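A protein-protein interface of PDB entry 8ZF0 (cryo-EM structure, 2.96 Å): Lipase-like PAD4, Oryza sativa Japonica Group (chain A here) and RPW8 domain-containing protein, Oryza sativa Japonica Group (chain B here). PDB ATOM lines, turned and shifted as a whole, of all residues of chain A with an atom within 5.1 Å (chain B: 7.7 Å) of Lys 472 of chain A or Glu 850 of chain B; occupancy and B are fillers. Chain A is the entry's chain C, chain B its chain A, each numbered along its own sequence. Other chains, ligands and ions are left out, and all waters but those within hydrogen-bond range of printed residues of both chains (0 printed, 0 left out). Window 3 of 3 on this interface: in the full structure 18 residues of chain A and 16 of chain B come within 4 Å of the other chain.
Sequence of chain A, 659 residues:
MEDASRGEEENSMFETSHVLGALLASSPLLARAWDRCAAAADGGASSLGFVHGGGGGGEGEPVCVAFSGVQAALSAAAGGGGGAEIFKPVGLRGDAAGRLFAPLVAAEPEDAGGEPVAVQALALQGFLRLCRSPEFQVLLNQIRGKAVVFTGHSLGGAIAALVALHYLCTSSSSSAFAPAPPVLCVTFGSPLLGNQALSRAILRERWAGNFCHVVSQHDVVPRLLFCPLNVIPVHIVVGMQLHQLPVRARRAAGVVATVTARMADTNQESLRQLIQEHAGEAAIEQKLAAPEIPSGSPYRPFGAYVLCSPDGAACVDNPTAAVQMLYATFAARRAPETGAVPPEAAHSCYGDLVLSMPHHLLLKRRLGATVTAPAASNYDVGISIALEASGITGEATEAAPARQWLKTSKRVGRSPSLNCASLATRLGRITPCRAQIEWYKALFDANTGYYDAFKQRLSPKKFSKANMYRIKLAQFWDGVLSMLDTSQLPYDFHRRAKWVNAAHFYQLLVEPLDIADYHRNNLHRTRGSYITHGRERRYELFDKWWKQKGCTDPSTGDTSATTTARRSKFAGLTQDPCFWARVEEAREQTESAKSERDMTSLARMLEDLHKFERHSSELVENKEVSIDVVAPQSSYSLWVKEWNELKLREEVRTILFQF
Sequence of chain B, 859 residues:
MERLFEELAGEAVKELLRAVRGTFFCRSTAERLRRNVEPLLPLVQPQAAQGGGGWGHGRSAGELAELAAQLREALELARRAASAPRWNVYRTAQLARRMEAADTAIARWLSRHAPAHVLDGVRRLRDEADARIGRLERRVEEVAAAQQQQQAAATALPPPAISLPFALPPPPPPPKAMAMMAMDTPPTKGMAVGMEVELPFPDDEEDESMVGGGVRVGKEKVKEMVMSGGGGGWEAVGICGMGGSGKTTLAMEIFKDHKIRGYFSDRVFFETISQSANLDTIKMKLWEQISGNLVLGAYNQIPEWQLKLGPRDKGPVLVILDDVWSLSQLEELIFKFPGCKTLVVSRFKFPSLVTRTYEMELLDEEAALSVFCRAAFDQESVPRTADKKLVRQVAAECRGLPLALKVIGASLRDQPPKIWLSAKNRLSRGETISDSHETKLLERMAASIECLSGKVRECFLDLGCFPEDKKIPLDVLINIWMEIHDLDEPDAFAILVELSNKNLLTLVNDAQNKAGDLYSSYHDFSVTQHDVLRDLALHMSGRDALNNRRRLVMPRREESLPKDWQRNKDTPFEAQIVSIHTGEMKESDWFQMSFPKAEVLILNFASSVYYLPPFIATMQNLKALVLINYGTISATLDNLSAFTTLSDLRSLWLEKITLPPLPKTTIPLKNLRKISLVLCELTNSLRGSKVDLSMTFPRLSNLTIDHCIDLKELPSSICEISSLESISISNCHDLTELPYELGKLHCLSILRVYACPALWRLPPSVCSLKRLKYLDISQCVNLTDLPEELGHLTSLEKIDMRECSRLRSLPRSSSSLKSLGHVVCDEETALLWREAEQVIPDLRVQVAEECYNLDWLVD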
ATOM      1  N   CYS A 433      22.595  11.509 -16.157  1.00  0.00           N
ATOM      2  CA  CYS A 433      21.416  11.924 -16.910  1.00  0.00           C
ATOM      3  C   CYS A 433      20.205  12.057 -15.992  1.00  0.00           C
ATOM      4  O   CYS A 433      19.437  13.023 -16.092  1.00  0.00           O
ATOM      5  CB  CYS A 433      21.133  10.931 -18.036  1.00  0.00           C
ATOM      6  SG  CYS A 433      22.520  10.663 -19.162  1.00  0.00           S
ATOM      7  N   ASN A 467      14.387  15.719 -22.879  1.00  0.00           N
ATOM      8  CA  ASN A 467      13.946  14.633 -23.747  1.00  0.00           C
ATOM      9  C   ASN A 467      15.110  13.731 -24.137  1.00  0.00           C
ATOM     10  O   ASN A 467      14.963  12.505 -24.187  1.00  0.00           O
ATOM     11  CB  ASN A 467      13.267  15.204 -24.993  1.00  0.00           C
ATOM     12  CG  ASN A 467      12.401  14.185 -25.703  1.00  0.00           C
ATOM     13  OD1 ASN A 467      11.456  13.646 -25.127  1.00  0.00           O
ATOM     14  ND2 ASN A 467      12.717  13.916 -26.965  1.00  0.00           N
ATOM     15  N   MET A 468      16.273  14.321 -24.422  1.00  0.00           N
ATOM     16  CA  MET A 468      17.453  13.524 -24.752  1.00  0.00           C
ATOM     17  C   MET A 468      17.830  12.604 -23.598  1.00  0.00           C
ATOM     18  O   MET A 468      18.086  11.408 -23.796  1.00  0.00           O
ATOM     19  CB  MET A 468      18.619  14.447 -25.103  1.00  0.00           C
ATOM     20  CG  MET A 468      18.921  14.552 -26.586  1.00  0.00           C
ATOM     21  SD  MET A 468      19.584  13.019 -27.261  1.00  0.00           S
ATOM     22  CE  MET A 468      18.635  12.885 -28.770  1.00  0.00           C
ATOM     23  N   TYR A 469      17.864  13.147 -22.380  1.00  0.00           N
ATOM     24  CA  TYR A 469      18.220  12.331 -21.223  1.00  0.00           C
ATOM     25  C   TYR A 469      17.180  11.244 -20.967  1.00  0.00           C
ATOM     26  O   TYR A 469      17.532  10.110 -20.618  1.00  0.00           O
ATOM     27  CB  TYR A 469      18.400  13.215 -19.992  1.00  0.00           C
ATOM     28  CG  TYR A 469      19.642  14.076 -20.050  1.00  0.00           C
ATOM     29  CD1 TYR A 469      20.844  13.558 -20.511  1.00  0.00           C
ATOM     30  CD2 TYR A 469      19.612  15.404 -19.649  1.00  0.00           C
ATOM     31  CE1 TYR A 469      21.984  14.337 -20.570  1.00  0.00           C
ATOM     32  CE2 TYR A 469      20.746  16.191 -19.704  1.00  0.00           C
ATOM     33  CZ  TYR A 469      21.928  15.653 -20.165  1.00  0.00           C
ATOM     34  OH  TYR A 469      23.060  16.433 -20.221  1.00  0.00           O
ATOM     35  N   ARG A 470      15.896  11.571 -21.138  1.00  0.00           N
ATOM     36  CA  ARG A 470      14.848  10.570 -20.967  1.00  0.00           C
ATOM     37  C   ARG A 470      14.988   9.444 -21.982  1.00  0.00           C
ATOM     38  O   ARG A 470      14.839   8.266 -21.638  1.00  0.00           O
ATOM     39  CB  ARG A 470      13.473  11.228 -21.081  1.00  0.00           C
ATOM     40  CG  ARG A 470      12.312  10.250 -21.033  1.00  0.00           C
ATOM     41  CD  ARG A 470      11.029  10.890 -21.535  1.00  0.00           C
ATOM     42  NE  ARG A 470      11.147  11.339 -22.917  1.00  0.00           N
ATOM     43  CZ  ARG A 470      10.433  10.857 -23.925  1.00  0.00           C
ATOM     44  NH1 ARG A 470       9.536   9.902 -23.742  1.00  0.00           N
ATOM     45  NH2 ARG A 470      10.624  11.345 -25.147  1.00  0.00           N
ATOM     46  N   ILE A 471      15.277   9.788 -23.240  1.00  0.00           N
ATOM     47  CA  ILE A 471      15.454   8.770 -24.272  1.00  0.00           C
ATOM     48  C   ILE A 471      16.653   7.888 -23.953  1.00  0.00           C
ATOM     49  O   ILE A 471      16.598   6.662 -24.110  1.00  0.00           O
ATOM     50  CB  ILE A 471      15.583   9.428 -25.659  1.00  0.00           C
ATOM     51  CG1 ILE A 471      14.252  10.057 -26.075  1.00  0.00           C
ATOM     52  CG2 ILE A 471      16.036   8.414 -26.696  1.00  0.00           C
ATOM     53  CD1 ILE A 471      14.323  10.832 -27.371  1.00  0.00           C
ATOM     54  N   LYS A 472      17.757   8.493 -23.505  1.00  0.00           N
ATOM     55  CA  LYS A 472      18.935   7.700 -23.158  1.00  0.00           C
ATOM     56  C   LYS A 472      18.644   6.746 -22.004  1.00  0.00           C
ATOM     57  O   LYS A 472      19.030   5.570 -22.047  1.00  0.00           O
ATOM     58  CB  LYS A 472      20.105   8.621 -22.813  1.00  0.00           C
ATOM     59  CG  LYS A 472      20.641   9.410 -23.996  1.00  0.00           C
ATOM     60  CD  LYS A 472      21.827  10.271 -23.595  1.00  0.00           C
ATOM     61  CE  LYS A 472      22.350  11.071 -24.775  1.00  0.00           C
ATOM     62  NZ  LYS A 472      23.509  11.926 -24.397  1.00  0.00           N
ATOM     63  N   LEU A 473      17.958   7.233 -20.964  1.00  0.00           N
ATOM     64  CA  LEU A 473      17.618   6.373 -19.835  1.00  0.00           C
ATOM     65  C   LEU A 473      16.695   5.238 -20.263  1.00  0.00           C
ATOM     66  O   LEU A 473      16.874   4.085 -19.843  1.00  0.00           O
ATOM     67  CB  LEU A 473      16.970   7.200 -18.725  1.00  0.00           C
ATOM     68  CG  LEU A 473      17.903   8.066 -17.877  1.00  0.00           C
ATOM     69  CD1 LEU A 473      17.114   9.126 -17.127  1.00  0.00           C
ATOM     70  CD2 LEU A 473      18.695   7.204 -16.909  1.00  0.00           C
ATOM     71  N   ALA A 474      15.699   5.546 -21.097  1.00  0.00           N
ATOM     72  CA  ALA A 474      14.783   4.516 -21.573  1.00  0.00           C
ATOM     73  C   ALA A 474      15.517   3.469 -22.397  1.00  0.00           C
ATOM     74  O   ALA A 474      15.252   2.270 -22.265  1.00  0.00           O
ATOM     75  CB  ALA A 474      13.657   5.150 -22.388  1.00  0.00           C
ATOM     76  N   GLN A 475      16.445   3.901 -23.256  1.00  0.00           N
ATOM     77  CA  GLN A 475      17.219   2.950 -24.046  1.00  0.00           C
ATOM     78  C   GLN A 475      18.077   2.060 -23.157  1.00  0.00           C
ATOM     79  O   GLN A 475      18.164   0.847 -23.382  1.00  0.00           O
ATOM     80  CB  GLN A 475      18.091   3.690 -25.059  1.00  0.00           C
ATOM     81  CG  GLN A 475      17.380   4.035 -26.356  1.00  0.00           C
ATOM     82  CD  GLN A 475      18.346   4.253 -27.502  1.00  0.00           C
ATOM     83  OE1 GLN A 475      19.562   4.165 -27.329  1.00  0.00           O
ATOM     84  NE2 GLN A 475      17.809   4.538 -28.682  1.00  0.00           N
ATOM     85  N   PHE A 476      18.718   2.643 -22.141  1.00  0.00           N
ATOM     86  CA  PHE A 476      19.546   1.845 -21.241  1.00  0.00           C
ATOM     87  C   PHE A 476      18.711   0.805 -20.501  1.00  0.00           C
ATOM     88  O   PHE A 476      19.097  -0.368 -20.400  1.00  0.00           O
ATOM     89  CB  PHE A 476      20.271   2.757 -20.250  1.00  0.00           C
ATOM     90  CG  PHE A 476      21.002   2.015 -19.168  1.00  0.00           C
ATOM     91  CD1 PHE A 476      22.121   1.256 -19.464  1.00  0.00           C
ATOM     92  CD2 PHE A 476      20.569   2.077 -17.854  1.00  0.00           C
ATOM     93  CE1 PHE A 476      22.795   0.572 -18.469  1.00  0.00           C
ATOM     94  CE2 PHE A 476      21.238   1.395 -16.855  1.00  0.00           C
ATOM     95  CZ  PHE A 476      22.353   0.643 -17.164  1.00  0.00           C
ATOM     96  N   TRP A 477      17.549   1.214 -19.988  1.00  0.00           N
ATOM     97  CA  TRP A 477      16.715   0.271 -19.247  1.00  0.00           C
ATOM     98  C   TRP A 477      16.112  -0.791 -20.163  1.00  0.00           C
ATOM     99  O   TRP A 477      15.968  -1.949 -19.754  1.00  0.00           O
ATOM    100  CB  TRP A 477      15.625   1.022 -18.486  1.00  0.00           C
ATOM    101  CG  TRP A 477      16.131   1.654 -17.224  1.00  0.00           C
ATOM    102  CD1 TRP A 477      16.183   2.987 -16.939  1.00  0.00           C
ATOM    103  CD2 TRP A 477      16.671   0.979 -16.081  1.00  0.00           C
ATOM    104  NE1 TRP A 477      16.715   3.184 -15.687  1.00  0.00           N
ATOM    105  CE2 TRP A 477      17.022   1.967 -15.140  1.00  0.00           C
ATOM    106  CE3 TRP A 477      16.888  -0.365 -15.760  1.00  0.00           C
ATOM    107  CZ2 TRP A 477      17.579   1.654 -13.901  1.00  0.00           C
ATOM    108  CZ3 TRP A 477      17.439  -0.673 -14.530  1.00  0.00           C
ATOM    109  CH2 TRP A 477      17.779   0.332 -13.616  1.00  0.00           C
ATOM    110  N   GLN B 512      32.857  19.940 -25.045  1.00  0.00           N
ATOM    111  CA  GLN B 512      32.955  18.714 -25.885  1.00  0.00           C
ATOM    112  C   GLN B 512      33.465  19.090 -27.275  1.00  0.00           C
ATOM    113  O   GLN B 512      32.769  18.776 -28.260  1.00  0.00           O
ATOM    114  CB  GLN B 512      31.581  18.058 -26.000  1.00  0.00           C
ATOM    115  CG  GLN B 512      30.795  18.059 -24.699  1.00  0.00           C
ATOM    116  CD  GLN B 512      29.393  17.534 -24.893  1.00  0.00           C
ATOM    117  OE1 GLN B 512      28.591  17.489 -23.962  1.00  0.00           O
ATOM    118  NE2 GLN B 512      29.084  17.139 -26.117  1.00  0.00           N
ATOM    119  N   GLN B 779      25.301  12.060 -31.774  1.00  0.00           N
ATOM    120  CA  GLN B 779      24.114  12.103 -30.922  1.00  0.00           C
ATOM    121  C   GLN B 779      22.869  11.565 -31.620  1.00  0.00           C
ATOM    122  O   GLN B 779      21.745  11.853 -31.197  1.00  0.00           O
ATOM    123  CB  GLN B 779      23.856  13.521 -30.397  1.00  0.00           C
ATOM    124  CG  GLN B 779      24.753  13.923 -29.239  1.00  0.00           C
ATOM    125  CD  GLN B 779      24.320  15.222 -28.588  1.00  0.00           C
ATOM    126  OE1 GLN B 779      24.307  16.276 -29.225  1.00  0.00           O
ATOM    127  NE2 GLN B 779      23.963  15.152 -27.311  1.00  0.00           N
ATOM    128  N   VAL B 781      20.818   8.892 -31.582  1.00  0.00           N
ATOM    129  CA  VAL B 781      20.613   7.757 -30.689  1.00  0.00           C
ATOM    130  C   VAL B 781      19.932   6.599 -31.406  1.00  0.00           C
ATOM    131  O   VAL B 781      20.226   5.431 -31.124  1.00  0.00           O
ATOM    132  CB  VAL B 781      19.814   8.197 -29.449  1.00  0.00           C
ATOM    133  CG1 VAL B 781      20.041   7.229 -28.303  1.00  0.00           C
ATOM    134  CG2 VAL B 781      20.208   9.607 -29.043  1.00  0.00           C
ATOM    135  N   ARG B 802      29.618  10.089 -32.652  1.00  0.00           N
ATOM    136  CA  ARG B 802      29.615   9.955 -31.204  1.00  0.00           C
ATOM    137  C   ARG B 802      28.193   9.780 -30.683  1.00  0.00           C
ATOM    138  O   ARG B 802      27.243  10.353 -31.222  1.00  0.00           O
ATOM    139  CB  ARG B 802      30.277  11.180 -30.568  1.00  0.00           C
ATOM    140  CG  ARG B 802      30.114  11.297 -29.062  1.00  0.00           C
ATOM    141  CD  ARG B 802      31.271  12.063 -28.438  1.00  0.00           C
ATOM    142  NE  ARG B 802      31.776  13.113 -29.315  1.00  0.00           N
ATOM    143  CZ  ARG B 802      31.225  14.313 -29.445  1.00  0.00           C
ATOM    144  NH1 ARG B 802      30.143  14.654 -28.764  1.00  0.00           N
ATOM    145  NH2 ARG B 802      31.774  15.192 -30.278  1.00  0.00           N
ATOM    146  N   GLU B 803      28.054   8.964 -29.634  1.00  0.00           N
ATOM    147  CA  GLU B 803      26.772   8.705 -28.974  1.00  0.00           C
ATOM    148  C   GLU B 803      25.765   8.038 -29.910  1.00  0.00           C
ATOM    149  O   GLU B 803      24.559   8.276 -29.811  1.00  0.00           O
ATOM    150  CB  GLU B 803      26.178   9.987 -28.381  1.00  0.00           C
ATOM    151  CG  GLU B 803      27.003  10.592 -27.257  1.00  0.00           C
ATOM    152  CD  GLU B 803      27.503   9.550 -26.277  1.00  0.00           C
ATOM    153  OE1 GLU B 803      26.665   8.881 -25.637  1.00  0.00           O
ATOM    154  OE2 GLU B 803      28.737   9.399 -26.146  1.00  0.00           O
ATOM    155  N   SER B 805      24.489   4.875 -30.041  1.00  0.00           N
ATOM    156  CA  SER B 805      24.375   3.602 -29.335  1.00  0.00           C
ATOM    157  C   SER B 805      23.742   2.525 -30.209  1.00  0.00           C
ATOM    158  O   SER B 805      24.187   1.372 -30.199  1.00  0.00           O
ATOM    159  CB  SER B 805      23.571   3.789 -28.048  1.00  0.00           C
ATOM    160  OG  SER B 805      22.311   4.380 -28.317  1.00  0.00           O
ATOM    161  N   ASP B 826      32.765   6.680 -30.192  1.00  0.00           N
ATOM    162  CA  ASP B 826      32.836   6.068 -28.874  1.00  0.00           C
ATOM    163  C   ASP B 826      33.695   4.805 -28.921  1.00  0.00           C
ATOM    164  O   ASP B 826      34.214   4.407 -29.968  1.00  0.00           O
ATOM    165  CB  ASP B 826      31.432   5.761 -28.356  1.00  0.00           C
ATOM    166  CG  ASP B 826      30.516   5.225 -29.438  1.00  0.00           C
ATOM    167  OD1 ASP B 826      30.827   4.159 -30.010  1.00  0.00           O
ATOM    168  OD2 ASP B 826      29.483   5.870 -29.717  1.00  0.00           O
ATOM    169  N   ALA B 848      36.020   9.347 -27.487  1.00  0.00           N
ATOM    170  CA  ALA B 848      35.524  10.479 -26.720  1.00  0.00           C
ATOM    171  C   ALA B 848      34.392  10.028 -25.808  1.00  0.00           C
ATOM    172  O   ALA B 848      33.535   9.237 -26.212  1.00  0.00           O
ATOM    173  CB  ALA B 848      35.040  11.605 -27.640  1.00  0.00           C
ATOM    174  N   GLU B 849      34.396  10.536 -24.580  1.00  0.00           N
ATOM    175  CA  GLU B 849      33.385  10.208 -23.587  1.00  0.00           C
ATOM    176  C   GLU B 849      32.417  11.372 -23.421  1.00  0.00           C
ATOM    177  O   GLU B 849      32.757  12.529 -23.686  1.00  0.00           O
ATOM    178  CB  GLU B 849      34.026   9.866 -22.239  1.00  0.00           C
ATOM    179  CG  GLU B 849      35.054   8.749 -22.306  1.00  0.00           C
ATOM    180  CD  GLU B 849      35.831   8.595 -21.013  1.00  0.00           C
ATOM    181  OE1 GLU B 849      36.502   9.564 -20.602  1.00  0.00           O
ATOM    182  OE2 GLU B 849      35.770   7.504 -20.409  1.00  0.00           O
ATOM    183  N   GLU B 850      31.203  11.052 -22.980  1.00  0.00           N
ATOM    184  CA  GLU B 850      30.184  12.073 -22.783  1.00  0.00           C
ATOM    185  C   GLU B 850      30.557  12.987 -21.623  1.00  0.00           C
ATOM    186  O   GLU B 850      31.061  12.538 -20.590  1.00  0.00           O
ATOM    187  CB  GLU B 850      28.826  11.423 -22.523  1.00  0.00           C
ATOM    188  CG  GLU B 850      27.646  12.369 -22.669  1.00  0.00           C
ATOM    189  CD  GLU B 850      26.311  11.659 -22.558  1.00  0.00           C
ATOM    190  OE1 GLU B 850      26.308  10.427 -22.353  1.00  0.00           O
ATOM    191  OE2 GLU B 850      25.267  12.332 -22.674  1.00  0.00           O
ATOM    192  N   CYS B 851      30.308  14.283 -21.801  1.00  0.00           N
ATOM    193  CA  CYS B 851      30.592  15.292 -20.791  1.00  0.00           C
ATOM    194  C   CYS B 851      29.291  15.968 -20.384  1.00  0.00           C
ATOM    195  O   CYS B 851      28.482  16.334 -21.242  1.00  0.00           O
ATOM    196  CB  CYS B 851      31.591  16.328 -21.310  1.00  0.00           C
ATOM    197  SG  CYS B 851      31.937  17.675 -20.155  1.00  0.00           S
ATOM    198  N   TYR B 852      29.093  16.129 -19.078  1.00  0.00           N
ATOM    199  CA  TYR B 852      27.884  16.722 -18.526  1.00  0.00           C
ATOM    200  C   TYR B 852      28.198  18.112 -17.991  1.00  0.00           C
ATOM    201  O   TYR B 852      29.164  18.291 -17.241  1.00  0.00           O
ATOM    202  CB  TYR B 852      27.303  15.841 -17.419  1.00  0.00           C
ATOM    203  CG  TYR B 852      27.010  14.427 -17.866  1.00  0.00           C
ATOM    204  CD1 TYR B 852      25.966  14.158 -18.743  1.00  0.00           C
ATOM    205  CD2 TYR B 852      27.781  13.363 -17.419  1.00  0.00           C
ATOM    206  CE1 TYR B 852      25.696  12.867 -19.156  1.00  0.00           C
ATOM    207  CE2 TYR B 852      27.519  12.070 -17.829  1.00  0.00           C
ATOM    208  CZ  TYR B 852      26.476  11.828 -18.697  1.00  0.00           C
ATOM    209  OH  TYR B 852      26.210  10.542 -19.106  1.00  0.00           O
ATOM    210  N   ASN B 853      27.353  19.084 -18.343  1.00  0.00           N
ATOM    211  CA  ASN B 853      27.547  20.487 -17.888  1.00  0.00           C
ATOM    212  C   ASN B 853      26.191  21.085 -17.514  1.00  0.00           C
ATOM    213  O   ASN B 853      25.167  20.447 -17.811  1.00  0.00           O
ATOM    214  CB  ASN B 853      28.208  21.346 -18.962  1.00  0.00           C
ATOM    215  CG  ASN B 853      27.403  21.423 -20.240  1.00  0.00           C
ATOM    216  OD1 ASN B 853      26.909  22.486 -20.604  1.00  0.00           O
ATOM    217  ND2 ASN B 853      27.253  20.302 -20.927  1.00  0.00           N
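Printed residues of chain B that touch a printed residue of chain A: Val 781, Ser 805, Glu 850 and Tyr 852. Among the printed residues, Asp or Glu carboxylates within 4 Å of a Lys or Arg side-chain nitrogen of the other chain: Lys 472 of chain A with Glu 850 of chain B (2.5 Å).
Met 468 of chain A touches Val 781 of chain B (CE to CG2, 3.6 Å). OH of Tyr 469 of chain A touches CD1 of Tyr 852 of chain B, at 3.98 Å. CG1 of Val 781 of chain B touches OE1 of Gln 475 of chain A, at 3.3 Å.
Of chain B, only Glu 850 comes within 4 Å of Lys 472 of chain A. Glu 850 of chain B touches just one residue of chain A: Lys 472. Of the printed residues of chain A, Val 781 of chain B touches Met 468 and Gln 475. Of the printed residues of chain B, Cys 433 of chain A touches Tyr 852 (3.7 Å). Of the printed residues of chain A, Tyr 852 of chain B touches Cys 433 and Tyr 469. The nearest residue of chain B that does not touch Lys 472 of chain A is Gln 779 of chain B (4.4 Å). The nearest residue of chain A that does not touch Glu 850 of chain B is Tyr 469 of chain A (4.4 Å).
The side-chain hydroxyl (OH) of Tyr 852 of chain B lies within hydrogen-bond range of the side-chain carboxylate (OE1) of Glu 850 of chain B (3.3 Å).
OE1 of Gln 475 of chain A sits at hydrogen-bond distance from OG of Ser 805 of chain B (2.9 Å). OH of Tyr 852 of chain B is in hydrogen-bond range of SG of Cys 433 of chain A, 3.7 Å away. The side-chain amino group (NZ) of Lys 472 of chain A lies within salt-bridge range of the side-chain carboxylate (OE2) of Glu 850 of chain B, at 2.5 Å.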
